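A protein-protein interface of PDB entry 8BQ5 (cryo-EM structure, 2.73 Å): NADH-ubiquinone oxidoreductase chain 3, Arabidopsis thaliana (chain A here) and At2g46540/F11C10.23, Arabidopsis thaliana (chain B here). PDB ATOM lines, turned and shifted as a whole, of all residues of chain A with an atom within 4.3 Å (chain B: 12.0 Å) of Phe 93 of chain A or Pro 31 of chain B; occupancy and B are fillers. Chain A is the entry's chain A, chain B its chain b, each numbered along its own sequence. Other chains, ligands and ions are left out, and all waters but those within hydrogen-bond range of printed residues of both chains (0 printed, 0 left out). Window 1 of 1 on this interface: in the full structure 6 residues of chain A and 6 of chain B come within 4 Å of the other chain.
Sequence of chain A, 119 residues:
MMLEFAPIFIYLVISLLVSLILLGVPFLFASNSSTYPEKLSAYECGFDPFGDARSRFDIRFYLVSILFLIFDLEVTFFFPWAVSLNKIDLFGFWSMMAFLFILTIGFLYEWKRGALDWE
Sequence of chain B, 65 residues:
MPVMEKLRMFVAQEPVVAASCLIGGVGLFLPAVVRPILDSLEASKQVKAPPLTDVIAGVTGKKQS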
ATOM      1  N   TRP A  81      35.090   0.346 -12.401  1.00  0.00           N
ATOM      2  CA  TRP A  81      33.840   0.936 -12.945  1.00  0.00           C
ATOM      3  C   TRP A  81      34.138   1.791 -14.165  1.00  0.00           C
ATOM      4  O   TRP A  81      33.419   1.664 -15.153  1.00  0.00           O
ATOM      5  CB  TRP A  81      33.179   1.777 -11.849  1.00  0.00           C
ATOM      6  CG  TRP A  81      31.904   2.451 -12.243  1.00  0.00           C
ATOM      7  CD1 TRP A  81      30.681   1.872 -12.410  1.00  0.00           C
ATOM      8  CD2 TRP A  81      31.717   3.855 -12.482  1.00  0.00           C
ATOM      9  NE1 TRP A  81      29.752   2.814 -12.756  1.00  0.00           N
ATOM     10  CE2 TRP A  81      30.357   4.041 -12.803  1.00  0.00           C
ATOM     11  CE3 TRP A  81      32.566   4.966 -12.466  1.00  0.00           C
ATOM     12  CZ2 TRP A  81      29.829   5.295 -13.098  1.00  0.00           C
ATOM     13  CZ3 TRP A  81      32.041   6.204 -12.754  1.00  0.00           C
ATOM     14  CH2 TRP A  81      30.693   6.363 -13.068  1.00  0.00           C
ATOM     15  N   ASP A  89      26.672  -0.552 -18.657  1.00  0.00           N
ATOM     16  CA  ASP A  89      25.607   0.300 -19.219  1.00  0.00           C
ATOM     17  C   ASP A  89      24.875   1.006 -18.072  1.00  0.00           C
ATOM     18  O   ASP A  89      25.521   1.518 -17.146  1.00  0.00           O
ATOM     19  CB  ASP A  89      24.726  -0.528 -20.125  1.00  0.00           C
ATOM     20  CG  ASP A  89      24.102   0.297 -21.231  1.00  0.00           C
ATOM     21  OD1 ASP A  89      24.190   1.542 -21.165  1.00  0.00           O
ATOM     22  OD2 ASP A  89      23.528  -0.294 -22.168  1.00  0.00           O
ATOM     23  N   LEU A  90      23.540   1.059 -18.110  1.00  0.00           N
ATOM     24  CA  LEU A  90      22.787   1.877 -17.163  1.00  0.00           C
ATOM     25  C   LEU A  90      22.790   1.273 -15.765  1.00  0.00           C
ATOM     26  O   LEU A  90      22.828   2.006 -14.770  1.00  0.00           O
ATOM     27  CB  LEU A  90      21.352   2.053 -17.655  1.00  0.00           C
ATOM     28  CG  LEU A  90      21.072   3.141 -18.686  1.00  0.00           C
ATOM     29  CD1 LEU A  90      19.579   3.215 -18.941  1.00  0.00           C
ATOM     30  CD2 LEU A  90      21.615   4.486 -18.225  1.00  0.00           C
ATOM     31  N   PHE A  91      22.723  -0.055 -15.668  1.00  0.00           N
ATOM     32  CA  PHE A  91      22.641  -0.706 -14.365  1.00  0.00           C
ATOM     33  C   PHE A  91      23.876  -0.418 -13.522  1.00  0.00           C
ATOM     34  O   PHE A  91      23.766  -0.053 -12.345  1.00  0.00           O
ATOM     35  CB  PHE A  91      22.457  -2.213 -14.545  1.00  0.00           C
ATOM     36  CG  PHE A  91      21.961  -2.918 -13.316  1.00  0.00           C
ATOM     37  CD1 PHE A  91      22.811  -3.164 -12.250  1.00  0.00           C
ATOM     38  CD2 PHE A  91      20.648  -3.342 -13.229  1.00  0.00           C
ATOM     39  CE1 PHE A  91      22.359  -3.812 -11.123  1.00  0.00           C
ATOM     40  CE2 PHE A  91      20.191  -3.993 -12.103  1.00  0.00           C
ATOM     41  CZ  PHE A  91      21.047  -4.227 -11.049  1.00  0.00           C
ATOM     42  N   GLY A  92      25.065  -0.596 -14.101  1.00  0.00           N
ATOM     43  CA  GLY A  92      26.284  -0.339 -13.353  1.00  0.00           C
ATOM     44  C   GLY A  92      26.434   1.122 -12.982  1.00  0.00           C
ATOM     45  O   GLY A  92      26.904   1.454 -11.887  1.00  0.00           O
ATOM     46  N   PHE A  93      26.024   2.012 -13.885  1.00  0.00           N
ATOM     47  CA  PHE A  93      26.061   3.440 -13.596  1.00  0.00           C
ATOM     48  C   PHE A  93      25.238   3.766 -12.354  1.00  0.00           C
ATOM     49  O   PHE A  93      25.706   4.467 -11.452  1.00  0.00           O
ATOM     50  CB  PHE A  93      25.560   4.225 -14.810  1.00  0.00           C
ATOM     51  CG  PHE A  93      25.463   5.700 -14.577  1.00  0.00           C
ATOM     52  CD1 PHE A  93      26.574   6.511 -14.730  1.00  0.00           C
ATOM     53  CD2 PHE A  93      24.263   6.279 -14.204  1.00  0.00           C
ATOM     54  CE1 PHE A  93      26.491   7.868 -14.511  1.00  0.00           C
ATOM     55  CE2 PHE A  93      24.176   7.636 -13.982  1.00  0.00           C
ATOM     56  CZ  PHE A  93      25.290   8.432 -14.139  1.00  0.00           C
ATOM     57  N   TRP A  94      24.020   3.228 -12.271  1.00  0.00           N
ATOM     58  CA  TRP A  94      23.149   3.558 -11.147  1.00  0.00           C
ATOM     59  C   TRP A  94      23.562   2.846  -9.865  1.00  0.00           C
ATOM     60  O   TRP A  94      23.367   3.387  -8.772  1.00  0.00           O
ATOM     61  CB  TRP A  94      21.698   3.244 -11.502  1.00  0.00           C
ATOM     62  CG  TRP A  94      21.143   4.213 -12.491  1.00  0.00           C
ATOM     63  CD1 TRP A  94      20.703   3.936 -13.751  1.00  0.00           C
ATOM     64  CD2 TRP A  94      20.991   5.626 -12.314  1.00  0.00           C
ATOM     65  NE1 TRP A  94      20.277   5.086 -14.366  1.00  0.00           N
ATOM     66  CE2 TRP A  94      20.443   6.138 -13.504  1.00  0.00           C
ATOM     67  CE3 TRP A  94      21.258   6.506 -11.260  1.00  0.00           C
ATOM     68  CZ2 TRP A  94      20.159   7.490 -13.673  1.00  0.00           C
ATOM     69  CZ3 TRP A  94      20.974   7.847 -11.430  1.00  0.00           C
ATOM     70  CH2 TRP A  94      20.432   8.326 -12.627  1.00  0.00           C
ATOM     71  N   SER A  95      24.129   1.642  -9.965  1.00  0.00           N
ATOM     72  CA  SER A  95      24.659   0.998  -8.767  1.00  0.00           C
ATOM     73  C   SER A  95      25.810   1.809  -8.179  1.00  0.00           C
ATOM     74  O   SER A  95      25.881   2.017  -6.958  1.00  0.00           O
ATOM     75  CB  SER A  95      25.099  -0.431  -9.088  1.00  0.00           C
ATOM     76  OG  SER A  95      26.237  -0.445  -9.929  1.00  0.00           O
ATOM     77  N   MET A  96      26.701   2.303  -9.041  1.00  0.00           N
ATOM     78  CA  MET A  96      27.790   3.196  -8.562  1.00  0.00           C
ATOM     79  C   MET A  96      27.167   4.464  -7.974  1.00  0.00           C
ATOM     80  O   MET A  96      27.643   4.913  -6.932  1.00  0.00           O
ATOM     81  CB  MET A  96      28.749   3.602  -9.682  1.00  0.00           C
ATOM     82  CG  MET A  96      29.857   4.536  -9.227  1.00  0.00           C
ATOM     83  SD  MET A  96      30.782   3.933  -7.789  1.00  0.00           S
ATOM     84  CE  MET A  96      31.914   2.791  -8.574  1.00  0.00           C
ATOM     85  N   MET A  97      26.137   5.005  -8.625  1.00  0.00           N
ATOM     86  CA  MET A  97      25.500   6.213  -8.112  1.00  0.00           C
ATOM     87  C   MET A  97      24.955   5.998  -6.704  1.00  0.00           C
ATOM     88  O   MET A  97      25.072   6.878  -5.848  1.00  0.00           O
ATOM     89  CB  MET A  97      24.383   6.663  -9.054  1.00  0.00           C
ATOM     90  CG  MET A  97      24.841   7.438 -10.286  1.00  0.00           C
ATOM     91  SD  MET A  97      26.389   8.346 -10.087  1.00  0.00           S
ATOM     92  CE  MET A  97      27.564   7.220 -10.838  1.00  0.00           C
ATOM     93  N   CYS B  21      26.870  21.012  -7.011  1.00  0.00           N
ATOM     94  CA  CYS B  21      25.525  20.457  -7.076  1.00  0.00           C
ATOM     95  C   CYS B  21      24.964  20.541  -8.487  1.00  0.00           C
ATOM     96  O   CYS B  21      24.369  19.579  -8.972  1.00  0.00           O
ATOM     97  CB  CYS B  21      24.606  21.166  -6.083  1.00  0.00           C
ATOM     98  SG  CYS B  21      25.059  20.918  -4.352  1.00  0.00           S
ATOM     99  N   LEU B  22      25.159  21.671  -9.169  1.00  0.00           N
ATOM    100  CA  LEU B  22      24.652  21.789 -10.535  1.00  0.00           C
ATOM    101  C   LEU B  22      25.358  20.828 -11.488  1.00  0.00           C
ATOM    102  O   LEU B  22      24.712  20.202 -12.337  1.00  0.00           O
ATOM    103  CB  LEU B  22      24.781  23.230 -11.028  1.00  0.00           C
ATOM    104  CG  LEU B  22      23.608  24.135 -10.648  1.00  0.00           C
ATOM    105  CD1 LEU B  22      23.834  25.551 -11.145  1.00  0.00           C
ATOM    106  CD2 LEU B  22      22.295  23.576 -11.187  1.00  0.00           C
ATOM    107  N   ILE B  23      26.680  20.691 -11.361  1.00  0.00           N
ATOM    108  CA  ILE B  23      27.430  19.823 -12.267  1.00  0.00           C
ATOM    109  C   ILE B  23      27.008  18.368 -12.080  1.00  0.00           C
ATOM    110  O   ILE B  23      26.681  17.658 -13.045  1.00  0.00           O
ATOM    111  CB  ILE B  23      28.942  20.020 -12.048  1.00  0.00           C
ATOM    112  CG1 ILE B  23      29.394  21.344 -12.666  1.00  0.00           C
ATOM    113  CG2 ILE B  23      29.738  18.868 -12.625  1.00  0.00           C
ATOM    114  CD1 ILE B  23      30.710  21.846 -12.130  1.00  0.00           C
ATOM    115  N   GLY B  24      26.969  17.912 -10.824  1.00  0.00           N
ATOM    116  CA  GLY B  24      26.512  16.559 -10.556  1.00  0.00           C
ATOM    117  C   GLY B  24      25.050  16.352 -10.902  1.00  0.00           C
ATOM    118  O   GLY B  24      24.649  15.266 -11.321  1.00  0.00           O
ATOM    119  N   GLY B  25      24.231  17.390 -10.730  1.00  0.00           N
ATOM    120  CA  GLY B  25      22.827  17.273 -11.072  1.00  0.00           C
ATOM    121  C   GLY B  25      22.613  17.101 -12.559  1.00  0.00           C
ATOM    122  O   GLY B  25      21.753  16.333 -12.979  1.00  0.00           O
ATOM    123  N   VAL B  26      23.389  17.818 -13.374  1.00  0.00           N
ATOM    124  CA  VAL B  26      23.348  17.596 -14.818  1.00  0.00           C
ATOM    125  C   VAL B  26      23.779  16.170 -15.137  1.00  0.00           C
ATOM    126  O   VAL B  26      23.140  15.466 -15.937  1.00  0.00           O
ATOM    127  CB  VAL B  26      24.228  18.631 -15.544  1.00  0.00           C
ATOM    128  CG1 VAL B  26      24.609  18.129 -16.926  1.00  0.00           C
ATOM    129  CG2 VAL B  26      23.515  19.967 -15.639  1.00  0.00           C
ATOM    130  N   GLY B  27      24.865  15.720 -14.499  1.00  0.00           N
ATOM    131  CA  GLY B  27      25.344  14.365 -14.727  1.00  0.00           C
ATOM    132  C   GLY B  27      24.350  13.285 -14.342  1.00  0.00           C
ATOM    133  O   GLY B  27      24.365  12.194 -14.915  1.00  0.00           O
ATOM    134  N   LEU B  28      23.501  13.555 -13.353  1.00  0.00           N
ATOM    135  CA  LEU B  28      22.463  12.604 -12.964  1.00  0.00           C
ATOM    136  C   LEU B  28      21.195  12.759 -13.794  1.00  0.00           C
ATOM    137  O   LEU B  28      20.479  11.779 -14.026  1.00  0.00           O
ATOM    138  CB  LEU B  28      22.125  12.764 -11.481  1.00  0.00           C
ATOM    139  CG  LEU B  28      23.256  12.482 -10.495  1.00  0.00           C
ATOM    140  CD1 LEU B  28      22.950  13.104  -9.144  1.00  0.00           C
ATOM    141  CD2 LEU B  28      23.473  10.987 -10.365  1.00  0.00           C
ATOM    142  N   PHE B  29      20.912  13.979 -14.246  1.00  0.00           N
ATOM    143  CA  PHE B  29      19.679  14.255 -14.967  1.00  0.00           C
ATOM    144  C   PHE B  29      19.738  13.710 -16.385  1.00  0.00           C
ATOM    145  O   PHE B  29      18.723  13.255 -16.924  1.00  0.00           O
ATOM    146  CB  PHE B  29      19.419  15.762 -14.968  1.00  0.00           C
ATOM    147  CG  PHE B  29      18.257  16.183 -15.814  1.00  0.00           C
ATOM    148  CD1 PHE B  29      16.971  16.168 -15.302  1.00  0.00           C
ATOM    149  CD2 PHE B  29      18.449  16.610 -17.117  1.00  0.00           C
ATOM    150  CE1 PHE B  29      15.900  16.561 -16.077  1.00  0.00           C
ATOM    151  CE2 PHE B  29      17.382  17.000 -17.897  1.00  0.00           C
ATOM    152  CZ  PHE B  29      16.105  16.976 -17.376  1.00  0.00           C
ATOM    153  N   LEU B  30      20.916  13.751 -17.008  1.00  0.00           N
ATOM    154  CA  LEU B  30      21.016  13.253 -18.379  1.00  0.00           C
ATOM    155  C   LEU B  30      20.644  11.778 -18.511  1.00  0.00           C
ATOM    156  O   LEU B  30      19.797  11.458 -19.364  1.00  0.00           O
ATOM    157  CB  LEU B  30      22.411  13.543 -18.937  1.00  0.00           C
ATOM    158  CG  LEU B  30      22.625  15.014 -19.297  1.00  0.00           C
ATOM    159  CD1 LEU B  30      24.099  15.317 -19.493  1.00  0.00           C
ATOM    160  CD2 LEU B  30      21.818  15.394 -20.527  1.00  0.00           C
ATOM    161  N   PRO B  31      21.181  10.844 -17.717  1.00  0.00           N
ATOM    162  CA  PRO B  31      20.791   9.439 -17.919  1.00  0.00           C
ATOM    163  C   PRO B  31      19.414   9.104 -17.372  1.00  0.00           C
ATOM    164  O   PRO B  31      18.787   8.154 -17.858  1.00  0.00           O
ATOM    165  CB  PRO B  31      21.890   8.652 -17.194  1.00  0.00           C
ATOM    166  CG  PRO B  31      22.456   9.588 -16.211  1.00  0.00           C
ATOM    167  CD  PRO B  31      22.208  10.985 -16.672  1.00  0.00           C
ATOM    168  N   ALA B  32      18.925   9.843 -16.376  1.00  0.00           N
ATOM    169  CA  ALA B  32      17.622   9.529 -15.797  1.00  0.00           C
ATOM    170  C   ALA B  32      16.481  10.005 -16.690  1.00  0.00           C
ATOM    171  O   ALA B  32      15.396   9.411 -16.686  1.00  0.00           O
ATOM    172  CB  ALA B  32      17.502  10.144 -14.404  1.00  0.00           C
ATOM    173  N   VAL B  33      16.696  11.068 -17.456  1.00  0.00           N
ATOM    174  CA  VAL B  33      15.648  11.690 -18.254  1.00  0.00           C
ATOM    175  C   VAL B  33      15.948  11.598 -19.746  1.00  0.00           C
ATOM    176  O   VAL B  33      15.136  11.094 -20.521  1.00  0.00           O
ATOM    177  CB  VAL B  33      15.423  13.158 -17.827  1.00  0.00           C
ATOM    178  CG1 VAL B  33      14.434  13.830 -18.767  1.00  0.00           C
ATOM    179  CG2 VAL B  33      14.935  13.223 -16.392  1.00  0.00           C
ATOM    180  N   VAL B  34      17.104  12.108 -20.170  1.00  0.00           N
ATOM    181  CA  VAL B  34      17.395  12.190 -21.596  1.00  0.00           C
ATOM    182  C   VAL B  34      17.607  10.801 -22.189  1.00  0.00           C
ATOM    183  O   VAL B  34      17.123  10.504 -23.287  1.00  0.00           O
ATOM    184  CB  VAL B  34      18.608  13.109 -21.831  1.00  0.00           C
ATOM    185  CG1 VAL B  34      19.039  13.065 -23.285  1.00  0.00           C
ATOM    186  CG2 VAL B  34      18.270  14.531 -21.415  1.00  0.00           C
ATOM    187  N   ARG B  35      18.320   9.927 -21.478  1.00  0.00           N
ATOM    188  CA  ARG B  35      18.601   8.596 -22.013  1.00  0.00           C
ATOM    189  C   ARG B  35      17.342   7.781 -22.286  1.00  0.00           C
ATOM    190  O   ARG B  35      17.259   7.167 -23.364  1.00  0.00           O
ATOM    191  CB  ARG B  35      19.564   7.857 -21.079  1.00  0.00           C
ATOM    192  CG  ARG B  35      19.705   6.375 -21.377  1.00  0.00           C
ATOM    193  CD  ARG B  35      20.388   6.129 -22.712  1.00  0.00           C
ATOM    194  NE  ARG B  35      20.545   4.704 -22.967  1.00  0.00           N
ATOM    195  CZ  ARG B  35      21.708   4.069 -22.972  1.00  0.00           C
ATOM    196  NH1 ARG B  35      22.848   4.714 -22.787  1.00  0.00           N
ATOM    197  NH2 ARG B  35      21.729   2.753 -23.165  1.00  0.00           N
ATOM    198  N   PRO B  36      16.352   7.699 -21.387  1.00  0.00           N
ATOM    199  CA  PRO B  36      15.097   7.032 -21.773  1.00  0.00           C
ATOM    200  C   PRO B  36      14.378   7.723 -22.917  1.00  0.00           C
ATOM    201  O   PRO B  36      13.697   7.052 -23.700  1.00  0.00           O
ATOM    202  CB  PRO B  36      14.268   7.052 -20.480  1.00  0.00           C
ATOM    203  CG  PRO B  36      14.867   8.105 -19.649  1.00  0.00           C
ATOM    204  CD  PRO B  36      16.328   8.093 -19.967  1.00  0.00           C
ATOM    205  N   ILE B  37      14.508   9.045 -23.040  1.00  0.00           N
ATOM    206  CA  ILE B  37      13.896   9.751 -24.163  1.00  0.00           C
ATOM    207  C   ILE B  37      14.526   9.305 -25.478  1.00  0.00           C
ATOM    208  O   ILE B  37      13.831   9.076 -26.475  1.00  0.00           O
ATOM    209  CB  ILE B  37      14.007  11.273 -23.964  1.00  0.00           C
ATOM    210  CG1 ILE B  37      13.037  11.729 -22.871  1.00  0.00           C
ATOM    211  CG2 ILE B  37      13.735  12.009 -25.267  1.00  0.00           C
ATOM    212  CD1 ILE B  37      12.966  13.228 -22.698  1.00  0.00           C
ATOM    213  N   LEU B  38      15.856   9.174 -25.500  1.00  0.00           N
ATOM    214  CA  LEU B  38      16.523   8.697 -26.708  1.00  0.00           C
ATOM    215  C   LEU B  38      16.221   7.229 -26.973  1.00  0.00           C
ATOM    216  O   LEU B  38      16.088   6.825 -28.133  1.00  0.00           O
ATOM    217  CB  LEU B  38      18.034   8.914 -26.607  1.00  0.00           C
ATOM    218  CG  LEU B  38      18.525  10.314 -26.244  1.00  0.00           C
ATOM    219  CD1 LEU B  38      20.033  10.403 -26.398  1.00  0.00           C
ATOM    220  CD2 LEU B  38      17.833  11.372 -27.086  1.00  0.00           C
ATOM    221  N   ASP B  39      16.128   6.414 -25.919  1.00  0.00           N
ATOM    222  CA  ASP B  39      15.777   5.010 -26.106  1.00  0.00           C
ATOM    223  C   ASP B  39      14.388   4.870 -26.713  1.00  0.00           C
ATOM    224  O   ASP B  39      14.191   4.094 -27.655  1.00  0.00           O
ATOM    225  CB  ASP B  39      15.853   4.265 -24.775  1.00  0.00           C
ATOM    226  CG  ASP B  39      17.276   4.069 -24.298  1.00  0.00           C
ATOM    227  OD1 ASP B  39      18.203   4.508 -25.011  1.00  0.00           O
ATOM    228  OD2 ASP B  39      17.467   3.476 -23.215  1.00  0.00           O
ATOM    229  N   SER B  40      13.420   5.627 -26.193  1.00  0.00           N
ATOM    230  CA  SER B  40      12.060   5.575 -26.719  1.00  0.00           C
ATOM    231  C   SER B  40      12.002   6.067 -28.160  1.00  0.00           C
ATOM    232  O   SER B  40      11.284   5.496 -28.987  1.00  0.00           O
ATOM    233  CB  SER B  40      11.128   6.397 -25.829  1.00  0.00           C
ATOM    234  OG  SER B  40      11.661   7.686 -25.584  1.00  0.00           O
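Printed residues of chain B that touch a printed residue of chain A: Gly 27, Leu 28, Pro 31, Ala 32 and Arg 35. Hydrophobic or aromatic side chains of chain B within 4 Å of the printed part of chain A: Leu 28, Pro 31 and Ala 32. Of the 10 printed residues of chain A, 5 touch a printed residue of chain B. Printed residues of chain A that touch a printed residue of chain B: Asp 89, Leu 90, Phe 93, Trp 94 and Met 97. Hydrophobic or aromatic side chains of chain A within 4 Å of the printed part of chain B: Leu 90, Phe 93, Trp 94 and Met 97. Among the printed residues, 7 pairs touch across the chains. Among the printed residues, Asp or Glu carboxylates within 4 Å of a Lys or Arg side-chain nitrogen of the other chain: Asp 89 of chain A with Arg 35 of chain B.
The side-chain carboxylate (OD1) of Asp 89 of chain A lies within salt-bridge range of the guanidinium group (NH2) of Arg 35 of chain B, at 3.4 Å.
O of Leu 30 of chain B sits at hydrogen-bond distance from N of Arg 35 of chain B (3.0 Å). The guanidinium group (NE) of Arg 35 of chain B lies within salt-bridge range of the side-chain carboxylate (OD1) of Asp 39 of chain B, at 3.1 Å.
Of the printed residues of chain A, Pro 31 of chain B touches Phe 93 (3.4 Å). No residue of chain B comes within 4 Å of Gly 92 of chain A. No residue of chain B comes within 4 Å of Ser 95 of chain A. No residue of chain B comes within 4 Å of Met 96 of chain A. Met 97 of chain A touches just one residue of chain B: Leu 28. Of the printed residues of chain B, Asp 89 of chain A touches Arg 35 (3.4 Å). Printed residues of chain A within 4 Å of Leu 28 of chain B: Trp 94 and Met 97. Of the printed residues of chain A, Gly 27 of chain B touches Phe 93 (3.95 Å). Of the printed residues of chain A, Ala 32 of chain B touches Trp 94 (3.8 Å). Printed residues of chain B within 4 Å of Trp 94 of chain A: Leu 28 and Ala 32. The nearest residue of chain B that does not touch Phe 93 of chain A is Leu 28 of chain B (4.9 Å).
Leu 90 of chain A touches Arg 35 of chain B (CD1 to CG, 3.99 Å). Phe 93 of chain A touches Gly 27 of chain B. Phe 93 of chain A touches Pro 31 of chain B (CE2 to CG, 3.4 Å). Leu 28 of chain B touches Trp 94 of chain A. CZ2 of Trp 94 of chain A touches N of Ala 32 of chain B, 3.8 Å away. Met 97 of chain A touches Leu 28 of chain B (CG to CD2, 3.8 Å).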
